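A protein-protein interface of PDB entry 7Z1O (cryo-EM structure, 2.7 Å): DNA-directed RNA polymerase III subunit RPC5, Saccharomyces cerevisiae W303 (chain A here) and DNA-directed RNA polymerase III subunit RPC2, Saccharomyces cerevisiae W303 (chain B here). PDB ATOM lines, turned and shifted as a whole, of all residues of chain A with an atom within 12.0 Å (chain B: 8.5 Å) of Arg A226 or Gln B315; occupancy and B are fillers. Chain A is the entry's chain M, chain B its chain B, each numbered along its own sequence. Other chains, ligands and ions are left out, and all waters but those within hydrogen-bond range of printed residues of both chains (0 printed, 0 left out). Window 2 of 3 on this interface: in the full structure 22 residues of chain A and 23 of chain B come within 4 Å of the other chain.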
ATOM      1  N   SER A 223      10.935   5.938 -13.683  1.00  0.00           N
ATOM      2  CA  SER A 223      11.685   6.023 -14.932  1.00  0.00           C
ATOM      3  C   SER A 223      13.176   6.196 -14.665  1.00  0.00           C
ATOM      4  O   SER A 223      14.011   5.583 -15.330  1.00  0.00           O
ATOM      5  CB  SER A 223      11.166   7.178 -15.791  1.00  0.00           C
ATOM      6  OG  SER A 223      11.416   8.427 -15.171  1.00  0.00           O
ATOM      7  N   GLN A 224      13.503   7.035 -13.684  1.00  0.00           N
ATOM      8  CA  GLN A 224      14.888   7.300 -13.322  1.00  0.00           C
ATOM      9  C   GLN A 224      15.437   6.321 -12.293  1.00  0.00           C
ATOM     10  O   GLN A 224      16.607   6.437 -11.916  1.00  0.00           O
ATOM     11  CB  GLN A 224      15.029   8.734 -12.793  1.00  0.00           C
ATOM     12  CG  GLN A 224      14.248   9.015 -11.517  1.00  0.00           C
ATOM     13  CD  GLN A 224      15.105   8.914 -10.269  1.00  0.00           C
ATOM     14  OE1 GLN A 224      16.301   9.204 -10.298  1.00  0.00           O
ATOM     15  NE2 GLN A 224      14.494   8.500  -9.164  1.00  0.00           N
ATOM     16  N   ASN A 225      14.628   5.367 -11.831  1.00  0.00           N
ATOM     17  CA  ASN A 225      15.061   4.410 -10.811  1.00  0.00           C
ATOM     18  C   ASN A 225      15.661   3.173 -11.482  1.00  0.00           C
ATOM     19  O   ASN A 225      15.172   2.049 -11.363  1.00  0.00           O
ATOM     20  CB  ASN A 225      13.901   4.048  -9.895  1.00  0.00           C
ATOM     21  CG  ASN A 225      14.359   3.634  -8.510  1.00  0.00           C
ATOM     22  OD1 ASN A 225      15.434   4.027  -8.056  1.00  0.00           O
ATOM     23  ND2 ASN A 225      13.544   2.834  -7.831  1.00  0.00           N
ATOM     24  N   ARG A 226      16.754   3.409 -12.202  1.00  0.00           N
ATOM     25  CA  ARG A 226      17.510   2.344 -12.846  1.00  0.00           C
ATOM     26  C   ARG A 226      18.653   1.830 -11.982  1.00  0.00           C
ATOM     27  O   ARG A 226      19.442   1.005 -12.453  1.00  0.00           O
ATOM     28  CB  ARG A 226      18.063   2.826 -14.192  1.00  0.00           C
ATOM     29  CG  ARG A 226      17.367   2.229 -15.403  1.00  0.00           C
ATOM     30  CD  ARG A 226      16.011   2.870 -15.641  1.00  0.00           C
ATOM     31  NE  ARG A 226      15.474   2.533 -16.954  1.00  0.00           N
ATOM     32  CZ  ARG A 226      14.268   2.880 -17.381  1.00  0.00           C
ATOM     33  NH1 ARG A 226      13.440   3.579 -16.623  1.00  0.00           N
ATOM     34  NH2 ARG A 226      13.883   2.517 -18.601  1.00  0.00           N
ATOM     35  N   LEU A 227      18.762   2.298 -10.740  1.00  0.00           N
ATOM     36  CA  LEU A 227      19.864   1.893  -9.879  1.00  0.00           C
ATOM     37  C   LEU A 227      19.698   0.444  -9.440  1.00  0.00           C
ATOM     38  O   LEU A 227      18.647   0.053  -8.927  1.00  0.00           O
ATOM     39  CB  LEU A 227      19.938   2.809  -8.657  1.00  0.00           C
ATOM     40  CG  LEU A 227      19.968   4.312  -8.929  1.00  0.00           C
ATOM     41  CD1 LEU A 227      19.987   5.091  -7.625  1.00  0.00           C
ATOM     42  CD2 LEU A 227      21.162   4.677  -9.794  1.00  0.00           C
ATOM     43  N   THR A 228      20.748  -0.350  -9.642  1.00  0.00           N
ATOM     44  CA  THR A 228      20.770  -1.743  -9.224  1.00  0.00           C
ATOM     45  C   THR A 228      22.117  -2.050  -8.586  1.00  0.00           C
ATOM     46  O   THR A 228      23.140  -1.466  -8.950  1.00  0.00           O
ATOM     47  CB  THR A 228      20.527  -2.707 -10.397  1.00  0.00           C
ATOM     48  OG1 THR A 228      21.374  -2.351 -11.497  1.00  0.00           O
ATOM     49  CG2 THR A 228      19.070  -2.672 -10.841  1.00  0.00           C
ATOM     50  N   GLY A 229      22.106  -2.971  -7.632  1.00  0.00           N
ATOM     51  CA  GLY A 229      23.335  -3.414  -6.997  1.00  0.00           C
ATOM     52  C   GLY A 229      23.674  -2.576  -5.781  1.00  0.00           C
ATOM     53  O   GLY A 229      22.850  -2.414  -4.882  1.00  0.00           O
ATOM     54  N   SER A 230      24.901  -2.047  -5.754  1.00  0.00           N
ATOM     55  CA  SER A 230      25.364  -1.302  -4.588  1.00  0.00           C
ATOM     56  C   SER A 230      24.669   0.047  -4.471  1.00  0.00           C
ATOM     57  O   SER A 230      24.427   0.529  -3.357  1.00  0.00           O
ATOM     58  CB  SER A 230      26.880  -1.120  -4.653  1.00  0.00           C
ATOM     59  OG  SER A 230      27.361  -0.467  -3.491  1.00  0.00           O
ATOM     60  N   LEU A 231      24.358   0.682  -5.605  1.00  0.00           N
ATOM     61  CA  LEU A 231      23.694   1.982  -5.570  1.00  0.00           C
ATOM     62  C   LEU A 231      22.297   1.877  -4.973  1.00  0.00           C
ATOM     63  O   LEU A 231      21.896   2.722  -4.162  1.00  0.00           O
ATOM     64  CB  LEU A 231      23.630   2.578  -6.975  1.00  0.00           C
ATOM     65  CG  LEU A 231      24.975   2.859  -7.640  1.00  0.00           C
ATOM     66  CD1 LEU A 231      24.780   3.606  -8.945  1.00  0.00           C
ATOM     67  CD2 LEU A 231      25.867   3.640  -6.699  1.00  0.00           C
ATOM     68  N   LEU A 232      21.545   0.846  -5.363  1.00  0.00           N
ATOM     69  CA  LEU A 232      20.213   0.643  -4.804  1.00  0.00           C
ATOM     70  C   LEU A 232      20.281   0.348  -3.313  1.00  0.00           C
ATOM     71  O   LEU A 232      19.455   0.844  -2.537  1.00  0.00           O
ATOM     72  CB  LEU A 232      19.501  -0.488  -5.544  1.00  0.00           C
ATOM     73  CG  LEU A 232      18.115  -0.879  -5.032  1.00  0.00           C
ATOM     74  CD1 LEU A 232      17.124   0.252  -5.252  1.00  0.00           C
ATOM     75  CD2 LEU A 232      17.636  -2.153  -5.706  1.00  0.00           C
ATOM     76  N   ALA A 233      21.263  -0.455  -2.893  1.00  0.00           N
ATOM     77  CA  ALA A 233      21.426  -0.756  -1.474  1.00  0.00           C
ATOM     78  C   ALA A 233      21.766   0.496  -0.677  1.00  0.00           C
ATOM     79  O   ALA A 233      21.213   0.718   0.406  1.00  0.00           O
ATOM     80  CB  ALA A 233      22.504  -1.822  -1.284  1.00  0.00           C
ATOM     81  N   HIS A 234      22.660   1.335  -1.203  1.00  0.00           N
ATOM     82  CA  HIS A 234      23.014   2.570  -0.511  1.00  0.00           C
ATOM     83  C   HIS A 234      21.829   3.527  -0.439  1.00  0.00           C
ATOM     84  O   HIS A 234      21.603   4.168   0.594  1.00  0.00           O
ATOM     85  CB  HIS A 234      24.203   3.235  -1.202  1.00  0.00           C
ATOM     86  CG  HIS A 234      25.530   2.816  -0.651  1.00  0.00           C
ATOM     87  ND1 HIS A 234      26.250   1.760  -1.167  1.00  0.00           N
ATOM     88  CD2 HIS A 234      26.267   3.308   0.372  1.00  0.00           C
ATOM     89  CE1 HIS A 234      27.373   1.621  -0.486  1.00  0.00           C
ATOM     90  NE2 HIS A 234      27.408   2.548   0.453  1.00  0.00           N
ATOM     91  N   LYS A 235      21.057   3.632  -1.525  1.00  0.00           N
ATOM     92  CA  LYS A 235      19.893   4.513  -1.528  1.00  0.00           C
ATOM     93  C   LYS A 235      18.830   4.033  -0.546  1.00  0.00           C
ATOM     94  O   LYS A 235      18.240   4.835   0.188  1.00  0.00           O
ATOM     95  CB  LYS A 235      19.316   4.616  -2.939  1.00  0.00           C
ATOM     96  CG  LYS A 235      18.207   5.644  -3.074  1.00  0.00           C
ATOM     97  CD  LYS A 235      17.706   5.735  -4.505  1.00  0.00           C
ATOM     98  CE  LYS A 235      16.789   4.572  -4.839  1.00  0.00           C
ATOM     99  NZ  LYS A 235      15.556   4.586  -4.007  1.00  0.00           N
ATOM    100  N   VAL A 236      18.575   2.722  -0.511  1.00  0.00           N
ATOM    101  CA  VAL A 236      17.546   2.208   0.387  1.00  0.00           C
ATOM    102  C   VAL A 236      18.034   2.234   1.831  1.00  0.00           C
ATOM    103  O   VAL A 236      17.222   2.279   2.763  1.00  0.00           O
ATOM    104  CB  VAL A 236      17.093   0.799  -0.050  1.00  0.00           C
ATOM    105  CG1 VAL A 236      18.132  -0.255   0.290  1.00  0.00           C
ATOM    106  CG2 VAL A 236      15.742   0.449   0.561  1.00  0.00           C
ATOM    107  N   GLU A 239      17.530   6.064   2.738  1.00  0.00           N
ATOM    108  CA  GLU A 239      16.123   6.427   2.875  1.00  0.00           C
ATOM    109  C   GLU A 239      15.497   5.784   4.108  1.00  0.00           C
ATOM    110  O   GLU A 239      14.482   6.270   4.621  1.00  0.00           O
ATOM    111  CB  GLU A 239      15.354   6.023   1.618  1.00  0.00           C
ATOM    112  CG  GLU A 239      15.391   7.051   0.503  1.00  0.00           C
ATOM    113  CD  GLU A 239      14.906   6.488  -0.817  1.00  0.00           C
ATOM    114  OE1 GLU A 239      15.223   7.078  -1.871  1.00  0.00           O
ATOM    115  OE2 GLU A 239      14.205   5.454  -0.801  1.00  0.00           O
ATOM    116  N   LEU B  84      15.543  -4.423 -23.094  1.00  0.00           N
ATOM    117  CA  LEU B  84      14.422  -3.616 -22.635  1.00  0.00           C
ATOM    118  C   LEU B  84      14.325  -2.371 -23.502  1.00  0.00           C
ATOM    119  O   LEU B  84      15.334  -1.705 -23.754  1.00  0.00           O
ATOM    120  CB  LEU B  84      14.582  -3.223 -21.163  1.00  0.00           C
ATOM    121  CG  LEU B  84      14.178  -4.233 -20.086  1.00  0.00           C
ATOM    122  CD1 LEU B  84      15.220  -5.330 -19.924  1.00  0.00           C
ATOM    123  CD2 LEU B  84      13.934  -3.529 -18.762  1.00  0.00           C
ATOM    124  N   SER B  85      13.114  -2.062 -23.956  1.00  0.00           N
ATOM    125  CA  SER B  85      12.893  -0.886 -24.786  1.00  0.00           C
ATOM    126  C   SER B  85      12.704   0.344 -23.908  1.00  0.00           C
ATOM    127  O   SER B  85      11.969   0.305 -22.917  1.00  0.00           O
ATOM    128  CB  SER B  85      11.673  -1.087 -25.683  1.00  0.00           C
ATOM    129  OG  SER B  85      11.427   0.064 -26.472  1.00  0.00           O
ATOM    130  N   ASP B  86      13.374   1.438 -24.275  1.00  0.00           N
ATOM    131  CA  ASP B  86      13.204   2.686 -23.539  1.00  0.00           C
ATOM    132  C   ASP B  86      11.850   3.318 -23.836  1.00  0.00           C
ATOM    133  O   ASP B  86      11.322   4.088 -23.025  1.00  0.00           O
ATOM    134  CB  ASP B  86      14.336   3.654 -23.881  1.00  0.00           C
ATOM    135  CG  ASP B  86      15.697   3.127 -23.475  1.00  0.00           C
ATOM    136  OD1 ASP B  86      16.289   2.348 -24.251  1.00  0.00           O
ATOM    137  OD2 ASP B  86      16.175   3.491 -22.381  1.00  0.00           O
ATOM    138  N   VAL B  87      11.278   3.010 -25.004  1.00  0.00           N
ATOM    139  CA  VAL B  87       9.994   3.590 -25.388  1.00  0.00           C
ATOM    140  C   VAL B  87       8.868   3.036 -24.524  1.00  0.00           C
ATOM    141  O   VAL B  87       8.040   3.790 -23.999  1.00  0.00           O
ATOM    142  CB  VAL B  87       9.729   3.347 -26.885  1.00  0.00           C
ATOM    143  CG1 VAL B  87       8.455   4.052 -27.322  1.00  0.00           C
ATOM    144  CG2 VAL B  87      10.915   3.809 -27.715  1.00  0.00           C
ATOM    145  N   ASP B  88       8.819   1.716 -24.357  1.00  0.00           N
ATOM    146  CA  ASP B  88       7.721   1.066 -23.667  1.00  0.00           C
ATOM    147  C   ASP B  88       8.251   0.262 -22.486  1.00  0.00           C
ATOM    148  O   ASP B  88       9.025  -0.685 -22.686  1.00  0.00           O
ATOM    149  CB  ASP B  88       6.948   0.147 -24.629  1.00  0.00           C
ATOM    150  CG  ASP B  88       5.572  -0.221 -24.110  1.00  0.00           C
ATOM    151  OD1 ASP B  88       5.227   0.177 -22.979  1.00  0.00           O
ATOM    152  OD2 ASP B  88       4.828  -0.907 -24.842  1.00  0.00           O
ATOM    153  N   PRO B  89       7.881   0.616 -21.250  1.00  0.00           N
ATOM    154  CA  PRO B  89       8.399  -0.128 -20.086  1.00  0.00           C
ATOM    155  C   PRO B  89       7.973  -1.587 -20.033  1.00  0.00           C
ATOM    156  O   PRO B  89       8.712  -2.416 -19.486  1.00  0.00           O
ATOM    157  CB  PRO B  89       7.845   0.662 -18.890  1.00  0.00           C
ATOM    158  CG  PRO B  89       6.753   1.524 -19.444  1.00  0.00           C
ATOM    159  CD  PRO B  89       7.130   1.818 -20.856  1.00  0.00           C
ATOM    160  N   THR B 311      34.296   8.109 -16.491  1.00  0.00           N
ATOM    161  CA  THR B 311      33.279   7.212 -17.024  1.00  0.00           C
ATOM    162  C   THR B 311      32.008   7.980 -17.368  1.00  0.00           C
ATOM    163  O   THR B 311      31.488   8.753 -16.560  1.00  0.00           O
ATOM    164  CB  THR B 311      32.961   6.107 -16.015  1.00  0.00           C
ATOM    165  OG1 THR B 311      34.173   5.452 -15.622  1.00  0.00           O
ATOM    166  CG2 THR B 311      32.012   5.084 -16.617  1.00  0.00           C
ATOM    167  N   MET B 312      31.510   7.758 -18.581  1.00  0.00           N
ATOM    168  CA  MET B 312      30.272   8.363 -19.048  1.00  0.00           C
ATOM    169  C   MET B 312      29.190   7.296 -19.112  1.00  0.00           C
ATOM    170  O   MET B 312      29.399   6.227 -19.692  1.00  0.00           O
ATOM    171  CB  MET B 312      30.470   9.015 -20.418  1.00  0.00           C
ATOM    172  CG  MET B 312      31.403  10.214 -20.394  1.00  0.00           C
ATOM    173  SD  MET B 312      31.575  11.006 -22.003  1.00  0.00           S
ATOM    174  CE  MET B 312      32.612   9.817 -22.850  1.00  0.00           C
ATOM    175  N   ARG B 313      28.038   7.589 -18.515  1.00  0.00           N
ATOM    176  CA  ARG B 313      26.964   6.620 -18.377  1.00  0.00           C
ATOM    177  C   ARG B 313      25.685   7.173 -18.986  1.00  0.00           C
ATOM    178  O   ARG B 313      25.542   8.380 -19.202  1.00  0.00           O
ATOM    179  CB  ARG B 313      26.731   6.252 -16.906  1.00  0.00           C
ATOM    180  CG  ARG B 313      26.370   4.796 -16.680  1.00  0.00           C
ATOM    181  CD  ARG B 313      27.617   3.933 -16.566  1.00  0.00           C
ATOM    182  NE  ARG B 313      28.607   4.518 -15.669  1.00  0.00           N
ATOM    183  CZ  ARG B 313      28.561   4.438 -14.347  1.00  0.00           C
ATOM    184  NH1 ARG B 313      27.579   3.805 -13.727  1.00  0.00           N
ATOM    185  NH2 ARG B 313      29.526   5.005 -13.629  1.00  0.00           N
ATOM    186  N   ARG B 314      24.755   6.259 -19.277  1.00  0.00           N
ATOM    187  CA  ARG B 314      23.460   6.655 -19.817  1.00  0.00           C
ATOM    188  C   ARG B 314      22.667   7.479 -18.810  1.00  0.00           C
ATOM    189  O   ARG B 314      22.052   8.490 -19.170  1.00  0.00           O
ATOM    190  CB  ARG B 314      22.668   5.416 -20.234  1.00  0.00           C
ATOM    191  CG  ARG B 314      21.280   5.711 -20.778  1.00  0.00           C
ATOM    192  CD  ARG B 314      21.345   6.403 -22.127  1.00  0.00           C
ATOM    193  NE  ARG B 314      20.016   6.716 -22.638  1.00  0.00           N
ATOM    194  CZ  ARG B 314      19.311   5.919 -23.429  1.00  0.00           C
ATOM    195  NH1 ARG B 314      19.779   4.747 -23.824  1.00  0.00           N
ATOM    196  NH2 ARG B 314      18.105   6.309 -23.833  1.00  0.00           N
ATOM    197  N   GLN B 315      22.673   7.067 -17.546  1.00  0.00           N
ATOM    198  CA  GLN B 315      21.905   7.741 -16.508  1.00  0.00           C
ATOM    199  C   GLN B 315      22.770   8.776 -15.802  1.00  0.00           C
ATOM    200  O   GLN B 315      23.974   8.572 -15.619  1.00  0.00           O
ATOM    201  CB  GLN B 315      21.356   6.729 -15.502  1.00  0.00           C
ATOM    202  CG  GLN B 315      22.417   5.883 -14.817  1.00  0.00           C
ATOM    203  CD  GLN B 315      21.830   4.903 -13.824  1.00  0.00           C
ATOM    204  OE1 GLN B 315      20.622   4.890 -13.586  1.00  0.00           O
ATOM    205  NE2 GLN B 315      22.684   4.072 -13.237  1.00  0.00           N
ATOM    206  N   LYS B 316      22.156   9.895 -15.426  1.00  0.00           N
ATOM    207  CA  LYS B 316      22.851  10.890 -14.623  1.00  0.00           C
ATOM    208  C   LYS B 316      22.984  10.392 -13.191  1.00  0.00           C
ATOM    209  O   LYS B 316      22.014   9.932 -12.582  1.00  0.00           O
ATOM    210  CB  LYS B 316      22.100  12.221 -14.654  1.00  0.00           C
ATOM    211  CG  LYS B 316      22.831  13.362 -13.969  1.00  0.00           C
ATOM    212  CD  LYS B 316      24.100  13.729 -14.721  1.00  0.00           C
ATOM    213  CE  LYS B 316      24.841  14.864 -14.034  1.00  0.00           C
ATOM    214  NZ  LYS B 316      24.077  16.140 -14.095  1.00  0.00           N
ATOM    215  N   LEU B 317      24.197  10.482 -12.650  1.00  0.00           N
ATOM    216  CA  LEU B 317      24.498   9.892 -11.356  1.00  0.00           C
ATOM    217  C   LEU B 317      25.043  10.952 -10.412  1.00  0.00           C
ATOM    218  O   LEU B 317      25.781  11.853 -10.818  1.00  0.00           O
ATOM    219  CB  LEU B 317      25.503   8.742 -11.483  1.00  0.00           C
ATOM    220  CG  LEU B 317      24.907   7.339 -11.612  1.00  0.00           C
ATOM    221  CD1 LEU B 317      26.009   6.307 -11.779  1.00  0.00           C
ATOM    222  CD2 LEU B 317      24.040   7.014 -10.409  1.00  0.00           C
ATOM    223  N   THR B 318      24.659  10.833  -9.144  1.00  0.00           N
ATOM    224  CA  THR B 318      25.214  11.670  -8.093  1.00  0.00           C
ATOM    225  C   THR B 318      26.701  11.359  -7.934  1.00  0.00           C
ATOM    226  O   THR B 318      27.144  10.230  -8.153  1.00  0.00           O
ATOM    227  CB  THR B 318      24.450  11.431  -6.784  1.00  0.00           C
ATOM    228  OG1 THR B 318      23.063  11.735  -6.985  1.00  0.00           O
ATOM    229  CG2 THR B 318      24.965  12.312  -5.649  1.00  0.00           C
ATOM    230  N   GLN B 321      27.249   8.710  -5.551  1.00  0.00           N
ATOM    231  CA  GLN B 321      26.840   7.469  -6.199  1.00  0.00           C
ATOM    232  C   GLN B 321      27.837   7.060  -7.272  1.00  0.00           C
ATOM    233  O   GLN B 321      28.113   5.869  -7.456  1.00  0.00           O
ATOM    234  CB  GLN B 321      25.446   7.624  -6.802  1.00  0.00           C
ATOM    235  CG  GLN B 321      24.335   7.777  -5.782  1.00  0.00           C
ATOM    236  CD  GLN B 321      22.965   7.817  -6.424  1.00  0.00           C
ATOM    237  OE1 GLN B 321      22.788   8.389  -7.500  1.00  0.00           O
ATOM    238  NE2 GLN B 321      21.985   7.207  -5.769  1.00  0.00           N
ATOM    239  N   GLU B 322      28.388   8.039  -7.992  1.00  0.00           N
ATOM    240  CA  GLU B 322      29.379   7.734  -9.015  1.00  0.00           C
ATOM    241  C   GLU B 322      30.646   7.163  -8.390  1.00  0.00           C
ATOM    242  O   GLU B 322      31.250   6.231  -8.933  1.00  0.00           O
ATOM    243  CB  GLU B 322      29.690   8.989  -9.829  1.00  0.00           C
ATOM    244  CG  GLU B 322      30.044   8.706 -11.275  1.00  0.00           C
ATOM    245  CD  GLU B 322      31.438   8.150 -11.436  1.00  0.00           C
ATOM    246  OE1 GLU B 322      32.310   8.506 -10.618  1.00  0.00           O
ATOM    247  OE2 GLU B 322      31.654   7.349 -12.370  1.00  0.00           O
ATOM    248  N   GLU B 325      29.911   3.589  -7.443  1.00  0.00           N
ATOM    249  CA  GLU B 325      29.951   2.740  -8.630  1.00  0.00           C
ATOM    250  C   GLU B 325      31.384   2.484  -9.079  1.00  0.00           C
ATOM    251  O   GLU B 325      31.723   1.369  -9.494  1.00  0.00           O
ATOM    252  CB  GLU B 325      29.140   3.376  -9.756  1.00  0.00           C
ATOM    253  CG  GLU B 325      28.955   2.481 -10.968  1.00  0.00           C
ATOM    254  CD  GLU B 325      28.032   1.308 -10.700  1.00  0.00           C
ATOM    255  OE1 GLU B 325      27.185   1.405  -9.787  1.00  0.00           O
ATOM    256  OE2 GLU B 325      28.150   0.286 -11.409  1.00  0.00           O
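O of Ser A223 sits at hydrogen-bond distance from NH1 of Arg A226, 2.5 Å away.
The side-chain hydroxyl (OG1) of Thr B318 is in hydrogen-bond range of the side-chain amide oxygen (OE1) of Gln B321 (3.4 Å).
Arg A226 touches Gln B315 (CB to OE1, 3.3 Å).
NE2 of Gln B315 touches CD2 of Leu A227, 3.8 Å away.
Leu A227 touches Leu B317.
Gln B321 touches Leu A227.
Leu A231 touches Leu B317 (CD1 to CD2, 3.8 Å).
Leu A231 touches Gln B321 (CD2 to O, 3.3 Å).
Leu A231 touches Glu B325 (CD1 to OE1, 3.4 Å).
Of chain B, only Gln B315 (3.3 Å) comes within 4 Å of Arg A226.
Gln B315 touches just these residues of chain A: Arg A226 (3.3 Å) and Leu A227 (3.8 Å).
No residue of chain A comes within 4 Å of Asp B86.
Arg B313 touches none of the printed residues of chain A.
No residue of chain A comes within 4 Å of Lys B316.
Leu B317 touches two residues of chain A.
Of the printed residues of chain A, Glu B325 touches Leu A231.
Printed residues of chain B within 4 Å of Leu A231: Leu B317, Gln B321 and Glu B325.
The nearest residue of chain A that does not touch Gln B315 is Gln A224 (4.6 Å).
Of the 15 printed residues of chain A, 3 touch a printed residue of chain B.
Hydrophobic or aromatic side chains of chain A within 4 Å of the printed part of chain B: Leu A227 and Leu A231.
Of the 17 printed residues of chain B, 4 touch a printed residue of chain A.
Among the printed residues, 7 pairs touch across the chains.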
